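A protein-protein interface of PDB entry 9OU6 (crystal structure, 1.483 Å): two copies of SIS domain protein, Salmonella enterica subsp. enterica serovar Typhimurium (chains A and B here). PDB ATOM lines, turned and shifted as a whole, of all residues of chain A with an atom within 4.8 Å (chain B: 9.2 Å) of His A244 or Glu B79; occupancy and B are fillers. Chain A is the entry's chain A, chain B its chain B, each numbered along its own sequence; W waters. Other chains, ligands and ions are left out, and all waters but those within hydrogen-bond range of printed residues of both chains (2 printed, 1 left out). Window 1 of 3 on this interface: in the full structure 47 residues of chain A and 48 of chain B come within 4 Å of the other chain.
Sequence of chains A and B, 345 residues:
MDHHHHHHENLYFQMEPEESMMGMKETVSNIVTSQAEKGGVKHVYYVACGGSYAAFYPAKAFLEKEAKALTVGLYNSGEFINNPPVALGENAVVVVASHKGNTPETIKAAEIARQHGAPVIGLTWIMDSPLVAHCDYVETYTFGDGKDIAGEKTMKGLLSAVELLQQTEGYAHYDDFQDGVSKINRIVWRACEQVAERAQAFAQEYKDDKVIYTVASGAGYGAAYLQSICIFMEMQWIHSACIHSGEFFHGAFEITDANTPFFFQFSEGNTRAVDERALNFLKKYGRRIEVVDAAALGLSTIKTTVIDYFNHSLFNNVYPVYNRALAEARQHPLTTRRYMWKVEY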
ATOM      1  N   VAL A 215     -32.750 -19.113 -18.438  1.00  0.00           N
ATOM      2  CA  VAL A 215     -31.876 -18.714 -17.363  1.00  0.00           C
ATOM      3  C   VAL A 215     -31.007 -19.904 -16.989  1.00  0.00           C
ATOM      4  O   VAL A 215     -31.550 -21.004 -16.760  1.00  0.00           O
ATOM      5  CB  VAL A 215     -32.639 -18.223 -16.119  1.00  0.00           C
ATOM      6  CG1 VAL A 215     -31.671 -17.709 -15.094  1.00  0.00           C
ATOM      7  CG2 VAL A 215     -33.714 -17.213 -16.451  1.00  0.00           C
ATOM      8  N   ALA A 216     -29.692 -19.727 -16.841  1.00  0.00           N
ATOM      9  CA  ALA A 216     -28.766 -20.767 -16.437  1.00  0.00           C
ATOM     10  C   ALA A 216     -27.452 -20.188 -15.945  1.00  0.00           C
ATOM     11  O   ALA A 216     -27.204 -18.993 -16.135  1.00  0.00           O
ATOM     12  CB  ALA A 216     -28.513 -21.758 -17.560  1.00  0.00           C
ATOM     13  N   SER A 217     -26.588 -21.043 -15.398  1.00  0.00           N
ATOM     14  CA  SER A 217     -25.230 -20.703 -15.029  1.00  0.00           C
ATOM     15  C   SER A 217     -24.348 -21.944 -15.065  1.00  0.00           C
ATOM     16  O   SER A 217     -24.844 -23.070 -15.121  1.00  0.00           O
ATOM     17  CB  SER A 217     -25.179 -20.003 -13.682  1.00  0.00           C
ATOM     18  OG  SER A 217     -25.412 -20.958 -12.631  1.00  0.00           O
ATOM     19  N   GLY A 218     -23.032 -21.735 -15.050  1.00  0.00           N
ATOM     20  CA  GLY A 218     -22.098 -22.829 -14.844  1.00  0.00           C
ATOM     21  C   GLY A 218     -21.837 -23.619 -16.120  1.00  0.00           C
ATOM     22  O   GLY A 218     -22.203 -23.206 -17.204  1.00  0.00           O
ATOM     23  N   TYR A 221     -24.367 -24.020 -19.105  1.00  0.00           N
ATOM     24  CA  TYR A 221     -24.968 -22.845 -19.717  1.00  0.00           C
ATOM     25  C   TYR A 221     -25.243 -23.047 -21.208  1.00  0.00           C
ATOM     26  O   TYR A 221     -26.228 -22.548 -21.730  1.00  0.00           O
ATOM     27  CB  TYR A 221     -24.046 -21.649 -19.445  1.00  0.00           C
ATOM     28  CG  TYR A 221     -24.632 -20.367 -19.994  1.00  0.00           C
ATOM     29  CD1 TYR A 221     -25.545 -19.568 -19.311  1.00  0.00           C
ATOM     30  CD2 TYR A 221     -24.290 -20.004 -21.272  1.00  0.00           C
ATOM     31  CE1 TYR A 221     -26.039 -18.399 -19.874  1.00  0.00           C
ATOM     32  CE2 TYR A 221     -24.793 -18.856 -21.851  1.00  0.00           C
ATOM     33  CZ  TYR A 221     -25.666 -18.063 -21.151  1.00  0.00           C
ATOM     34  OH  TYR A 221     -26.171 -16.965 -21.807  1.00  0.00           O
ATOM     35  N   CYS A 242     -30.670 -15.389 -23.289  1.00  0.00           N
ATOM     36  CA  CYS A 242     -30.327 -16.465 -22.396  1.00  0.00           C
ATOM     37  C   CYS A 242     -29.570 -15.835 -21.226  1.00  0.00           C
ATOM     38  O   CYS A 242     -28.465 -15.324 -21.421  1.00  0.00           O
ATOM     39  CB  CYS A 242     -29.497 -17.476 -23.166  1.00  0.00           C
ATOM     40  SG  CYS A 242     -29.020 -18.875 -22.121  1.00  0.00           S
ATOM     41  N   ILE A 243     -30.223 -15.711 -20.082  1.00  0.00           N
ATOM     42  CA  ILE A 243     -29.728 -14.882 -18.994  1.00  0.00           C
ATOM     43  C   ILE A 243     -28.869 -15.711 -18.057  1.00  0.00           C
ATOM     44  O   ILE A 243     -29.287 -16.764 -17.615  1.00  0.00           O
ATOM     45  CB  ILE A 243     -30.956 -14.350 -18.244  1.00  0.00           C
ATOM     46  CG1 ILE A 243     -31.929 -13.654 -19.179  1.00  0.00           C
ATOM     47  CG2 ILE A 243     -30.502 -13.483 -17.083  1.00  0.00           C
ATOM     48  CD1 ILE A 243     -33.318 -13.465 -18.629  1.00  0.00           C
ATOM     49  N   HIS A 244     -27.702 -15.224 -17.657  1.00  0.00           N
ATOM     50  CA  HIS A 244     -26.894 -15.847 -16.628  1.00  0.00           C
ATOM     51  C   HIS A 244     -27.518 -15.563 -15.268  1.00  0.00           C
ATOM     52  O   HIS A 244     -27.857 -14.428 -14.926  1.00  0.00           O
ATOM     53  CB  HIS A 244     -25.457 -15.306 -16.692  1.00  0.00           C
ATOM     54  CG  HIS A 244     -24.513 -16.010 -15.795  1.00  0.00           C
ATOM     55  ND1 HIS A 244     -24.502 -15.781 -14.435  1.00  0.00           N
ATOM     56  CD2 HIS A 244     -23.616 -16.971 -16.015  1.00  0.00           C
ATOM     57  CE1 HIS A 244     -23.585 -16.554 -13.885  1.00  0.00           C
ATOM     58  NE2 HIS A 244     -22.995 -17.247 -14.828  1.00  0.00           N
ATOM     59  N   SER A 245     -27.706 -16.642 -14.466  1.00  0.00           N
ATOM     60  CA  SER A 245     -28.322 -16.530 -13.161  1.00  0.00           C
ATOM     61  C   SER A 245     -27.680 -15.488 -12.260  1.00  0.00           C
ATOM     62  O   SER A 245     -28.345 -14.907 -11.408  1.00  0.00           O
ATOM     63  CB  SER A 245     -28.217 -17.851 -12.443  1.00  0.00           C
ATOM     64  OG  SER A 245     -28.860 -18.856 -13.183  1.00  0.00           O
ATOM     65  N   GLY A 246     -26.385 -15.324 -12.392  1.00  0.00           N
ATOM     66  CA  GLY A 246     -25.638 -14.430 -11.515  1.00  0.00           C
ATOM     67  C   GLY A 246     -25.812 -12.955 -11.839  1.00  0.00           C
ATOM     68  O   GLY A 246     -25.279 -12.117 -11.110  1.00  0.00           O
ATOM     69  N   GLU A 247     -26.536 -12.639 -12.906  1.00  0.00           N
ATOM     70  CA  GLU A 247     -26.699 -11.259 -13.331  1.00  0.00           C
ATOM     71  C   GLU A 247     -27.986 -10.609 -12.804  1.00  0.00           C
ATOM     72  O   GLU A 247     -28.132  -9.409 -13.012  1.00  0.00           O
ATOM     73  CB  GLU A 247     -26.627 -11.217 -14.843  1.00  0.00           C
ATOM     74  CG  GLU A 247     -25.203 -11.284 -15.374  1.00  0.00           C
ATOM     75  CD  GLU A 247     -24.451  -9.987 -14.983  1.00  0.00           C
ATOM     76  OE1 GLU A 247     -25.088  -8.899 -14.983  1.00  0.00           O
ATOM     77  OE2 GLU A 247     -23.265 -10.054 -14.598  1.00  0.00           O
ATOM     78  N   PHE A 248     -28.912 -11.379 -12.207  1.00  0.00           N
ATOM     79  CA  PHE A 248     -30.137 -10.813 -11.673  1.00  0.00           C
ATOM     80  C   PHE A 248     -29.787  -9.626 -10.778  1.00  0.00           C
ATOM     81  O   PHE A 248     -29.082  -9.800  -9.781  1.00  0.00           O
ATOM     82  CB  PHE A 248     -30.969 -11.862 -10.933  1.00  0.00           C
ATOM     83  CG  PHE A 248     -31.816 -12.597 -11.953  1.00  0.00           C
ATOM     84  CD1 PHE A 248     -31.245 -13.544 -12.785  1.00  0.00           C
ATOM     85  CD2 PHE A 248     -33.119 -12.207 -12.209  1.00  0.00           C
ATOM     86  CE1 PHE A 248     -31.992 -14.182 -13.754  1.00  0.00           C
ATOM     87  CE2 PHE A 248     -33.851 -12.817 -13.217  1.00  0.00           C
ATOM     88  CZ  PHE A 248     -33.280 -13.795 -14.000  1.00  0.00           C
ATOM     89  N   THR A 271     -22.529 -24.313  -9.039  1.00  0.00           N
ATOM     90  CA  THR A 271     -23.250 -23.069  -9.282  1.00  0.00           C
ATOM     91  C   THR A 271     -24.724 -23.174  -8.918  1.00  0.00           C
ATOM     92  O   THR A 271     -25.519 -22.259  -9.129  1.00  0.00           O
ATOM     93  CB  THR A 271     -23.063 -22.513 -10.710  1.00  0.00           C
ATOM     94  OG1 THR A 271     -23.723 -23.359 -11.657  1.00  0.00           O
ATOM     95  CG2 THR A 271     -21.575 -22.415 -11.030  1.00  0.00           C
ATOM     96  N   VAL A 274     -25.925 -20.167  -7.075  1.00  0.00           N
ATOM     97  CA  VAL A 274     -26.158 -19.017  -7.923  1.00  0.00           C
ATOM     98  C   VAL A 274     -27.555 -19.092  -8.519  1.00  0.00           C
ATOM     99  O   VAL A 274     -28.307 -18.114  -8.533  1.00  0.00           O
ATOM    100  CB  VAL A 274     -25.086 -18.932  -9.014  1.00  0.00           C
ATOM    101  CG1 VAL A 274     -25.274 -17.708  -9.882  1.00  0.00           C
ATOM    102  CG2 VAL A 274     -23.672 -18.917  -8.433  1.00  0.00           C
ATOM    103  N   VAL B  47     -13.138 -10.360 -12.823  1.00  0.00           N
ATOM    104  CA  VAL B  47     -14.302 -10.791 -12.074  1.00  0.00           C
ATOM    105  C   VAL B  47     -15.179  -9.557 -11.803  1.00  0.00           C
ATOM    106  O   VAL B  47     -14.782  -8.589 -11.167  1.00  0.00           O
ATOM    107  CB  VAL B  47     -13.933 -11.566 -10.798  1.00  0.00           C
ATOM    108  CG1 VAL B  47     -15.188 -12.075 -10.103  1.00  0.00           C
ATOM    109  CG2 VAL B  47     -12.941 -12.702 -11.019  1.00  0.00           C
ATOM    110  N   ALA B  48     -16.446  -9.625 -12.247  1.00  0.00           N
ATOM    111  CA  ALA B  48     -17.396  -8.540 -12.060  1.00  0.00           C
ATOM    112  C   ALA B  48     -18.808  -9.006 -12.355  1.00  0.00           C
ATOM    113  O   ALA B  48     -19.011 -10.117 -12.861  1.00  0.00           O
ATOM    114  CB  ALA B  48     -17.054  -7.326 -12.925  1.00  0.00           C
ATOM    115  N   CYS B  49     -19.763  -8.115 -12.080  1.00  0.00           N
ATOM    116  CA  CYS B  49     -21.154  -8.251 -12.484  1.00  0.00           C
ATOM    117  C   CYS B  49     -21.592  -7.037 -13.306  1.00  0.00           C
ATOM    118  O   CYS B  49     -20.957  -5.955 -13.322  1.00  0.00           O
ATOM    119  CB  CYS B  49     -22.114  -8.229 -11.299  1.00  0.00           C
ATOM    120  SG  CYS B  49     -21.708  -9.376  -9.983  1.00  0.00           S
ATOM    121  N   GLY B  50     -22.694  -7.220 -14.020  1.00  0.00           N
ATOM    122  CA  GLY B  50     -23.282  -6.099 -14.738  1.00  0.00           C
ATOM    123  C   GLY B  50     -22.377  -5.519 -15.798  1.00  0.00           C
ATOM    124  O   GLY B  50     -21.604  -6.183 -16.512  1.00  0.00           O
ATOM    125  N   TYR B  53     -18.748  -6.457 -16.022  1.00  0.00           N
ATOM    126  CA  TYR B  53     -18.334  -7.719 -16.607  1.00  0.00           C
ATOM    127  C   TYR B  53     -18.102  -7.537 -18.115  1.00  0.00           C
ATOM    128  O   TYR B  53     -17.082  -7.939 -18.666  1.00  0.00           O
ATOM    129  CB  TYR B  53     -19.396  -8.775 -16.313  1.00  0.00           C
ATOM    130  CG  TYR B  53     -19.214 -10.070 -17.058  1.00  0.00           C
ATOM    131  CD1 TYR B  53     -19.724 -10.254 -18.325  1.00  0.00           C
ATOM    132  CD2 TYR B  53     -18.538 -11.150 -16.493  1.00  0.00           C
ATOM    133  CE1 TYR B  53     -19.554 -11.441 -19.026  1.00  0.00           C
ATOM    134  CE2 TYR B  53     -18.344 -12.325 -17.184  1.00  0.00           C
ATOM    135  CZ  TYR B  53     -18.867 -12.496 -18.448  1.00  0.00           C
ATOM    136  OH  TYR B  53     -18.665 -13.670 -19.109  1.00  0.00           O
ATOM    137  N   LEU B  74     -12.664 -14.873 -17.490  1.00  0.00           N
ATOM    138  CA  LEU B  74     -13.615 -13.802 -17.204  1.00  0.00           C
ATOM    139  C   LEU B  74     -14.801 -14.474 -16.519  1.00  0.00           C
ATOM    140  O   LEU B  74     -15.431 -15.378 -17.120  1.00  0.00           O
ATOM    141  CB  LEU B  74     -13.986 -13.154 -18.535  1.00  0.00           C
ATOM    142  CG  LEU B  74     -15.151 -12.179 -18.509  1.00  0.00           C
ATOM    143  CD1 LEU B  74     -14.902 -11.046 -17.632  1.00  0.00           C
ATOM    144  CD2 LEU B  74     -15.471 -11.682 -19.945  1.00  0.00           C
ATOM    145  N   TYR B  75     -15.116 -13.974 -15.321  1.00  0.00           N
ATOM    146  CA  TYR B  75     -16.147 -14.578 -14.498  1.00  0.00           C
ATOM    147  C   TYR B  75     -17.166 -13.551 -14.080  1.00  0.00           C
ATOM    148  O   TYR B  75     -16.809 -12.466 -13.597  1.00  0.00           O
ATOM    149  CB  TYR B  75     -15.624 -15.201 -13.203  1.00  0.00           C
ATOM    150  CG  TYR B  75     -14.867 -16.505 -13.370  1.00  0.00           C
ATOM    151  CD1 TYR B  75     -13.564 -16.577 -13.815  1.00  0.00           C
ATOM    152  CD2 TYR B  75     -15.435 -17.695 -12.920  1.00  0.00           C
ATOM    153  CE1 TYR B  75     -12.850 -17.763 -13.870  1.00  0.00           C
ATOM    154  CE2 TYR B  75     -14.731 -18.883 -12.956  1.00  0.00           C
ATOM    155  CZ  TYR B  75     -13.442 -18.943 -13.449  1.00  0.00           C
ATOM    156  OH  TYR B  75     -12.822 -20.184 -13.450  1.00  0.00           O
ATOM    157  N   ASN B  76     -18.424 -13.989 -14.039  1.00  0.00           N
ATOM    158  CA  ASN B  76     -19.426 -13.372 -13.181  1.00  0.00           C
ATOM    159  C   ASN B  76     -19.065 -13.576 -11.699  1.00  0.00           C
ATOM    160  O   ASN B  76     -18.669 -14.654 -11.289  1.00  0.00           O
ATOM    161  CB  ASN B  76     -20.799 -14.006 -13.466  1.00  0.00           C
ATOM    162  CG  ASN B  76     -21.849 -13.573 -12.469  1.00  0.00           C
ATOM    163  OD1 ASN B  76     -22.473 -12.499 -12.609  1.00  0.00           O
ATOM    164  ND2 ASN B  76     -22.073 -14.391 -11.474  1.00  0.00           N
ATOM    165  N   SER B  77     -19.225 -12.540 -10.871  1.00  0.00           N
ATOM    166  CA  SER B  77     -18.758 -12.615  -9.497  1.00  0.00           C
ATOM    167  C   SER B  77     -19.443 -13.745  -8.746  1.00  0.00           C
ATOM    168  O   SER B  77     -18.782 -14.391  -7.949  1.00  0.00           O
ATOM    169  CB  SER B  77     -18.974 -11.309  -8.761  1.00  0.00           C
ATOM    170  OG  SER B  77     -18.364 -10.224  -9.438  1.00  0.00           O
ATOM    171  N   GLY B  78     -20.748 -13.909  -8.928  1.00  0.00           N
ATOM    172  CA  GLY B  78     -21.435 -15.009  -8.237  1.00  0.00           C
ATOM    173  C   GLY B  78     -20.897 -16.389  -8.601  1.00  0.00           C
ATOM    174  O   GLY B  78     -20.700 -17.286  -7.758  1.00  0.00           O
ATOM    175  N   GLU B  79     -20.662 -16.617  -9.878  1.00  0.00           N
ATOM    176  CA  GLU B  79     -20.080 -17.884 -10.313  1.00  0.00           C
ATOM    177  C   GLU B  79     -18.690 -18.056  -9.697  1.00  0.00           C
ATOM    178  O   GLU B  79     -18.300 -19.145  -9.274  1.00  0.00           O
ATOM    179  CB  GLU B  79     -20.105 -17.973 -11.830  1.00  0.00           C
ATOM    180  CG  GLU B  79     -19.464 -19.230 -12.387  1.00  0.00           C
ATOM    181  CD  GLU B  79     -19.913 -19.625 -13.778  1.00  0.00           C
ATOM    182  OE1 GLU B  79     -20.606 -18.846 -14.469  1.00  0.00           O
ATOM    183  OE2 GLU B  79     -19.440 -20.682 -14.226  1.00  0.00           O
ATOM    184  N   PHE B  80     -17.884 -16.986  -9.718  1.00  0.00           N
ATOM    185  CA  PHE B  80     -16.527 -17.094  -9.224  1.00  0.00           C
ATOM    186  C   PHE B  80     -16.479 -17.465  -7.740  1.00  0.00           C
ATOM    187  O   PHE B  80     -15.670 -18.321  -7.377  1.00  0.00           O
ATOM    188  CB  PHE B  80     -15.796 -15.770  -9.415  1.00  0.00           C
ATOM    189  CG  PHE B  80     -14.321 -15.736  -9.044  1.00  0.00           C
ATOM    190  CD1 PHE B  80     -13.373 -16.264  -9.898  1.00  0.00           C
ATOM    191  CD2 PHE B  80     -13.909 -15.195  -7.838  1.00  0.00           C
ATOM    192  CE1 PHE B  80     -12.030 -16.162  -9.605  1.00  0.00           C
ATOM    193  CE2 PHE B  80     -12.562 -15.158  -7.516  1.00  0.00           C
ATOM    194  CZ  PHE B  80     -11.645 -15.596  -8.423  1.00  0.00           C
ATOM    195  N   ILE B  81     -17.335 -16.867  -6.909  1.00  0.00           N
ATOM    196  CA  ILE B  81     -17.266 -17.135  -5.485  1.00  0.00           C
ATOM    197  C   ILE B  81     -17.818 -18.514  -5.137  1.00  0.00           C
ATOM    198  O   ILE B  81     -17.435 -19.073  -4.089  1.00  0.00           O
ATOM    199  CB  ILE B  81     -17.883 -16.007  -4.653  1.00  0.00           C
ATOM    200  CG1 ILE B  81     -19.381 -15.898  -4.844  1.00  0.00           C
ATOM    201  CG2 ILE B  81     -17.183 -14.676  -4.935  1.00  0.00           C
ATOM    202  CD1 ILE B  81     -20.041 -14.795  -4.054  1.00  0.00           C
ATOM    203  N   ASN B  82     -18.714 -19.038  -5.964  1.00  0.00           N
ATOM    204  CA  ASN B  82     -19.302 -20.349  -5.690  1.00  0.00           C
ATOM    205  C   ASN B  82     -18.481 -21.471  -6.293  1.00  0.00           C
ATOM    206  O   ASN B  82     -18.560 -22.643  -5.889  1.00  0.00           O
ATOM    207  CB  ASN B  82     -20.754 -20.391  -6.145  1.00  0.00           C
ATOM    208  CG  ASN B  82     -21.634 -19.682  -5.156  1.00  0.00           C
ATOM    209  OD1 ASN B  82     -22.071 -20.328  -4.185  1.00  0.00           O
ATOM    210  ND2 ASN B  82     -21.965 -18.420  -5.379  1.00  0.00           N
ATOM    211  N   ASN B  83     -17.718 -21.148  -7.343  1.00  0.00           N
ATOM    212  CA  ASN B  83     -16.986 -22.182  -8.051  1.00  0.00           C
ATOM    213  C   ASN B  83     -15.626 -21.662  -8.493  1.00  0.00           C
ATOM    214  O   ASN B  83     -15.285 -21.696  -9.685  1.00  0.00           O
ATOM    215  CB  ASN B  83     -17.746 -22.650  -9.282  1.00  0.00           C
ATOM    216  CG  ASN B  83     -17.211 -23.957  -9.826  1.00  0.00           C
ATOM    217  OD1 ASN B  83     -16.734 -24.819  -9.071  1.00  0.00           O
ATOM    218  ND2 ASN B  83     -17.368 -24.160 -11.120  1.00  0.00           N
ATOM    219  N   PRO B  84     -14.754 -21.256  -7.554  1.00  0.00           N
ATOM    220  CA  PRO B  84     -13.469 -20.678  -7.921  1.00  0.00           C
ATOM    221  C   PRO B  84     -12.567 -21.702  -8.605  1.00  0.00           C
ATOM    222  O   PRO B  84     -12.533 -22.873  -8.229  1.00  0.00           O
ATOM    223  CB  PRO B  84     -12.925 -20.181  -6.568  1.00  0.00           C
ATOM    224  CG  PRO B  84     -13.622 -21.008  -5.535  1.00  0.00           C
ATOM    225  CD  PRO B  84     -14.959 -21.306  -6.102  1.00  0.00           C
ATOM    226  N   PRO B  85     -11.769 -21.284  -9.594  1.00  0.00           N
ATOM    227  CA  PRO B  85     -10.866 -22.211 -10.274  1.00  0.00           C
ATOM    228  C   PRO B  85      -9.770 -22.736  -9.345  1.00  0.00           C
ATOM    229  O   PRO B  85      -9.365 -22.024  -8.401  1.00  0.00           O
ATOM    230  CB  PRO B  85     -10.275 -21.347 -11.379  1.00  0.00           C
ATOM    231  CG  PRO B  85     -10.346 -19.946 -10.835  1.00  0.00           C
ATOM    232  CD  PRO B  85     -11.618 -19.893 -10.013  1.00  0.00           C
ATOM    233  N   GLU B 105     -21.197  -9.616  -4.138  1.00  0.00           N
ATOM    234  CA  GLU B 105     -20.541 -10.776  -4.707  1.00  0.00           C
ATOM    235  C   GLU B 105     -19.123 -10.400  -5.114  1.00  0.00           C
ATOM    236  O   GLU B 105     -18.209 -11.242  -5.080  1.00  0.00           O
ATOM    237  CB  GLU B 105     -21.290 -11.377  -5.899  1.00  0.00           C
ATOM    238  CG  GLU B 105     -22.726 -11.796  -5.579  1.00  0.00           C
ATOM    239  CD  GLU B 105     -23.757 -10.705  -5.897  1.00  0.00           C
ATOM    240  OE1 GLU B 105     -24.711 -11.053  -6.620  1.00  0.00           O
ATOM    241  OE2 GLU B 105     -23.658  -9.531  -5.467  1.00  0.00           O
ATOM    242  N   THR B 106     -18.971  -9.179  -5.644  1.00  0.00           N
ATOM    243  CA  THR B 106     -17.652  -8.763  -6.114  1.00  0.00           C
ATOM    244  C   THR B 106     -16.689  -8.517  -4.953  1.00  0.00           C
ATOM    245  O   THR B 106     -15.509  -8.854  -4.986  1.00  0.00           O
ATOM    246  CB  THR B 106     -17.782  -7.520  -6.993  1.00  0.00           C
ATOM    247  OG1 THR B 106     -18.655  -7.874  -8.058  1.00  0.00           O
ATOM    248  CG2 THR B 106     -16.460  -7.170  -7.655  1.00  0.00           C
ATOM    249  N   ALA B 109     -15.598 -11.846  -3.937  1.00  0.00           N
ATOM    250  CA  ALA B 109     -14.583 -12.370  -4.832  1.00  0.00           C
ATOM    251  C   ALA B 109     -13.174 -11.883  -4.475  1.00  0.00           C
ATOM    252  O   ALA B 109     -12.186 -12.638  -4.464  1.00  0.00           O
ATOM    253  CB  ALA B 109     -14.972 -11.872  -6.229  1.00  0.00           C
ATOM    254  N   ILE B 112     -12.182 -13.793  -1.227  1.00  0.00           N
ATOM    255  CA  ILE B 112     -11.737 -15.153  -1.492  1.00  0.00           C
ATOM    256  C   ILE B 112     -10.383 -15.204  -2.187  1.00  0.00           C
ATOM    257  O   ILE B 112      -9.528 -16.025  -1.879  1.00  0.00           O
ATOM    258  CB  ILE B 112     -12.845 -15.928  -2.223  1.00  0.00           C
ATOM    259  CG1 ILE B 112     -14.049 -16.105  -1.293  1.00  0.00           C
ATOM    260  CG2 ILE B 112     -12.340 -17.273  -2.697  1.00  0.00           C
ATOM    261  CD1 ILE B 112     -15.290 -16.624  -1.984  1.00  0.00           C
ATOM    262  N   TYR B 225     -23.278  -6.021 -26.512  1.00  0.00           N
ATOM    263  CA  TYR B 225     -24.093  -6.645 -25.489  1.00  0.00           C
ATOM    264  C   TYR B 225     -24.679  -5.562 -24.587  1.00  0.00           C
ATOM    265  O   TYR B 225     -25.871  -5.520 -24.306  1.00  0.00           O
ATOM    266  CB  TYR B 225     -23.301  -7.628 -24.671  1.00  0.00           C
ATOM    267  CG  TYR B 225     -24.201  -8.225 -23.619  1.00  0.00           C
ATOM    268  CD1 TYR B 225     -25.092  -9.186 -24.056  1.00  0.00           C
ATOM    269  CD2 TYR B 225     -24.197  -7.847 -22.289  1.00  0.00           C
ATOM    270  CE1 TYR B 225     -26.014  -9.747 -23.195  1.00  0.00           C
ATOM    271  CE2 TYR B 225     -25.118  -8.416 -21.412  1.00  0.00           C
ATOM    272  CZ  TYR B 225     -26.025  -9.350 -21.886  1.00  0.00           C
ATOM    273  OH  TYR B 225     -26.997 -10.040 -21.206  1.00  0.00           O
ATOM    274  N   HIS B 239     -35.889  -8.196 -24.059  1.00  0.00           N
ATOM    275  CA  HIS B 239     -34.435  -8.185 -24.228  1.00  0.00           C
ATOM    276  C   HIS B 239     -34.082  -9.199 -25.296  1.00  0.00           C
ATOM    277  O   HIS B 239     -34.134 -10.401 -25.046  1.00  0.00           O
ATOM    278  CB  HIS B 239     -33.701  -8.502 -22.916  1.00  0.00           C
ATOM    279  CG  HIS B 239     -32.212  -8.403 -22.995  1.00  0.00           C
ATOM    280  ND1 HIS B 239     -31.351  -8.909 -22.050  1.00  0.00           N
ATOM    281  CD2 HIS B 239     -31.435  -7.759 -23.914  1.00  0.00           C
ATOM    282  CE1 HIS B 239     -30.088  -8.633 -22.402  1.00  0.00           C
ATOM    283  NE2 HIS B 239     -30.122  -7.923 -23.544  1.00  0.00           N
HETATM  284  O   HOH W   1     -21.719 -19.758 -16.858  1.00  0.00           O
HETATM  285  O   HOH W   2     -24.036 -12.708  -8.746  1.00  0.00           O
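The side-chain carboxylate (OE1) of Glu B79 sits at hydrogen-bond distance from a ring nitrogen (NE2) of His A244, 2.9 Å away.
The backbone carbonyl oxygen (O) of Gly A246 lies close to the side-chain amide oxygen (OD1) of Asn B76.
The backbone NH (N) of Gly B50 is in hydrogen-bond range of the side-chain carboxylate (OE2) of Glu A247, 2.9 Å away.
The side-chain carboxylate (OE2) of Glu A247 sits close to the side-chain amide oxygen (OD1) of Asn B76 (3.2 Å).
No position is printed for both chains.
Of the 9 pairs that touch across the chains among the printed residues, none has its exchanged pair printed and touching as well.
Water W2 lies within hydrogen-bond range of O of Gly A246 and OE1 of Glu B105.
Water W1 lies within hydrogen-bond range of the side-chain carboxylate (OE1) of Glu B79, the backbone NH (N) of Gly A218 and a ring nitrogen (NE2) of His A244.
Of the 23 printed residues of chain B, 6 touch a printed residue of chain A.
Of the 14 printed residues of chain A, 5 touch a printed residue of chain B.
Hydrophobic or aromatic side chains of chain A within 4 Å of the printed part of chain B: His A244 and Val A274.
Among the printed residues, no Asp or Glu carboxylate lies within 4 Å of a Lys or Arg side-chain nitrogen of the other chain.
Among the printed residues, merely in contact across the chains: Gly A218 with Glu B79, His A244 with Asn B76, Glu A247 with Cys B49, Val A274 with Gly B78 and Val A274 with Asn B82.
Of chain B, only Glu B79 (3.5 Å) comes within 4 Å of Gly A218.
Tyr A221 touches none of the printed residues of chain B.
His A244 touches just these residues of chain B: Asn B76 (3.6 Å) and Glu B79 (2.9 Å).
No residue of chain B comes within 4 Å of Ser A245.
Printed residues of chain B within 4 Å of Glu A247: Cys B49, Gly B50 and Asn B76.
Of the printed residues of chain B, Val A274 touches Gly B78 and Asn B82.
Glu B79 touches two residues of chain A.
Of the printed residues of chain A, Asn B82 touches Val A274 (3.5 Å).
The nearest residue of chain B that does not touch His A244 is Gly B78 (5.9 Å).
The backbone NH of Gly A246 lies within hydrogen-bond range of a ring nitrogen (ND1) of His A244.
The side-chain hydroxyl (OG) of Ser B77 is in hydrogen-bond range of the side-chain sulfur (SG) of Cys B49 (3.5 Å).
The side-chain amide nitrogen (ND2) of Asn B76 sits close to the backbone NH (N) of Gly B78, 2.9 Å away.
The backbone NH (N) of Glu B79 sits close to the side-chain amide nitrogen (ND2) of Asn B76, at 3.1 Å.
O of Gly B78 lies within hydrogen-bond range of ND2 of Asn B82.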
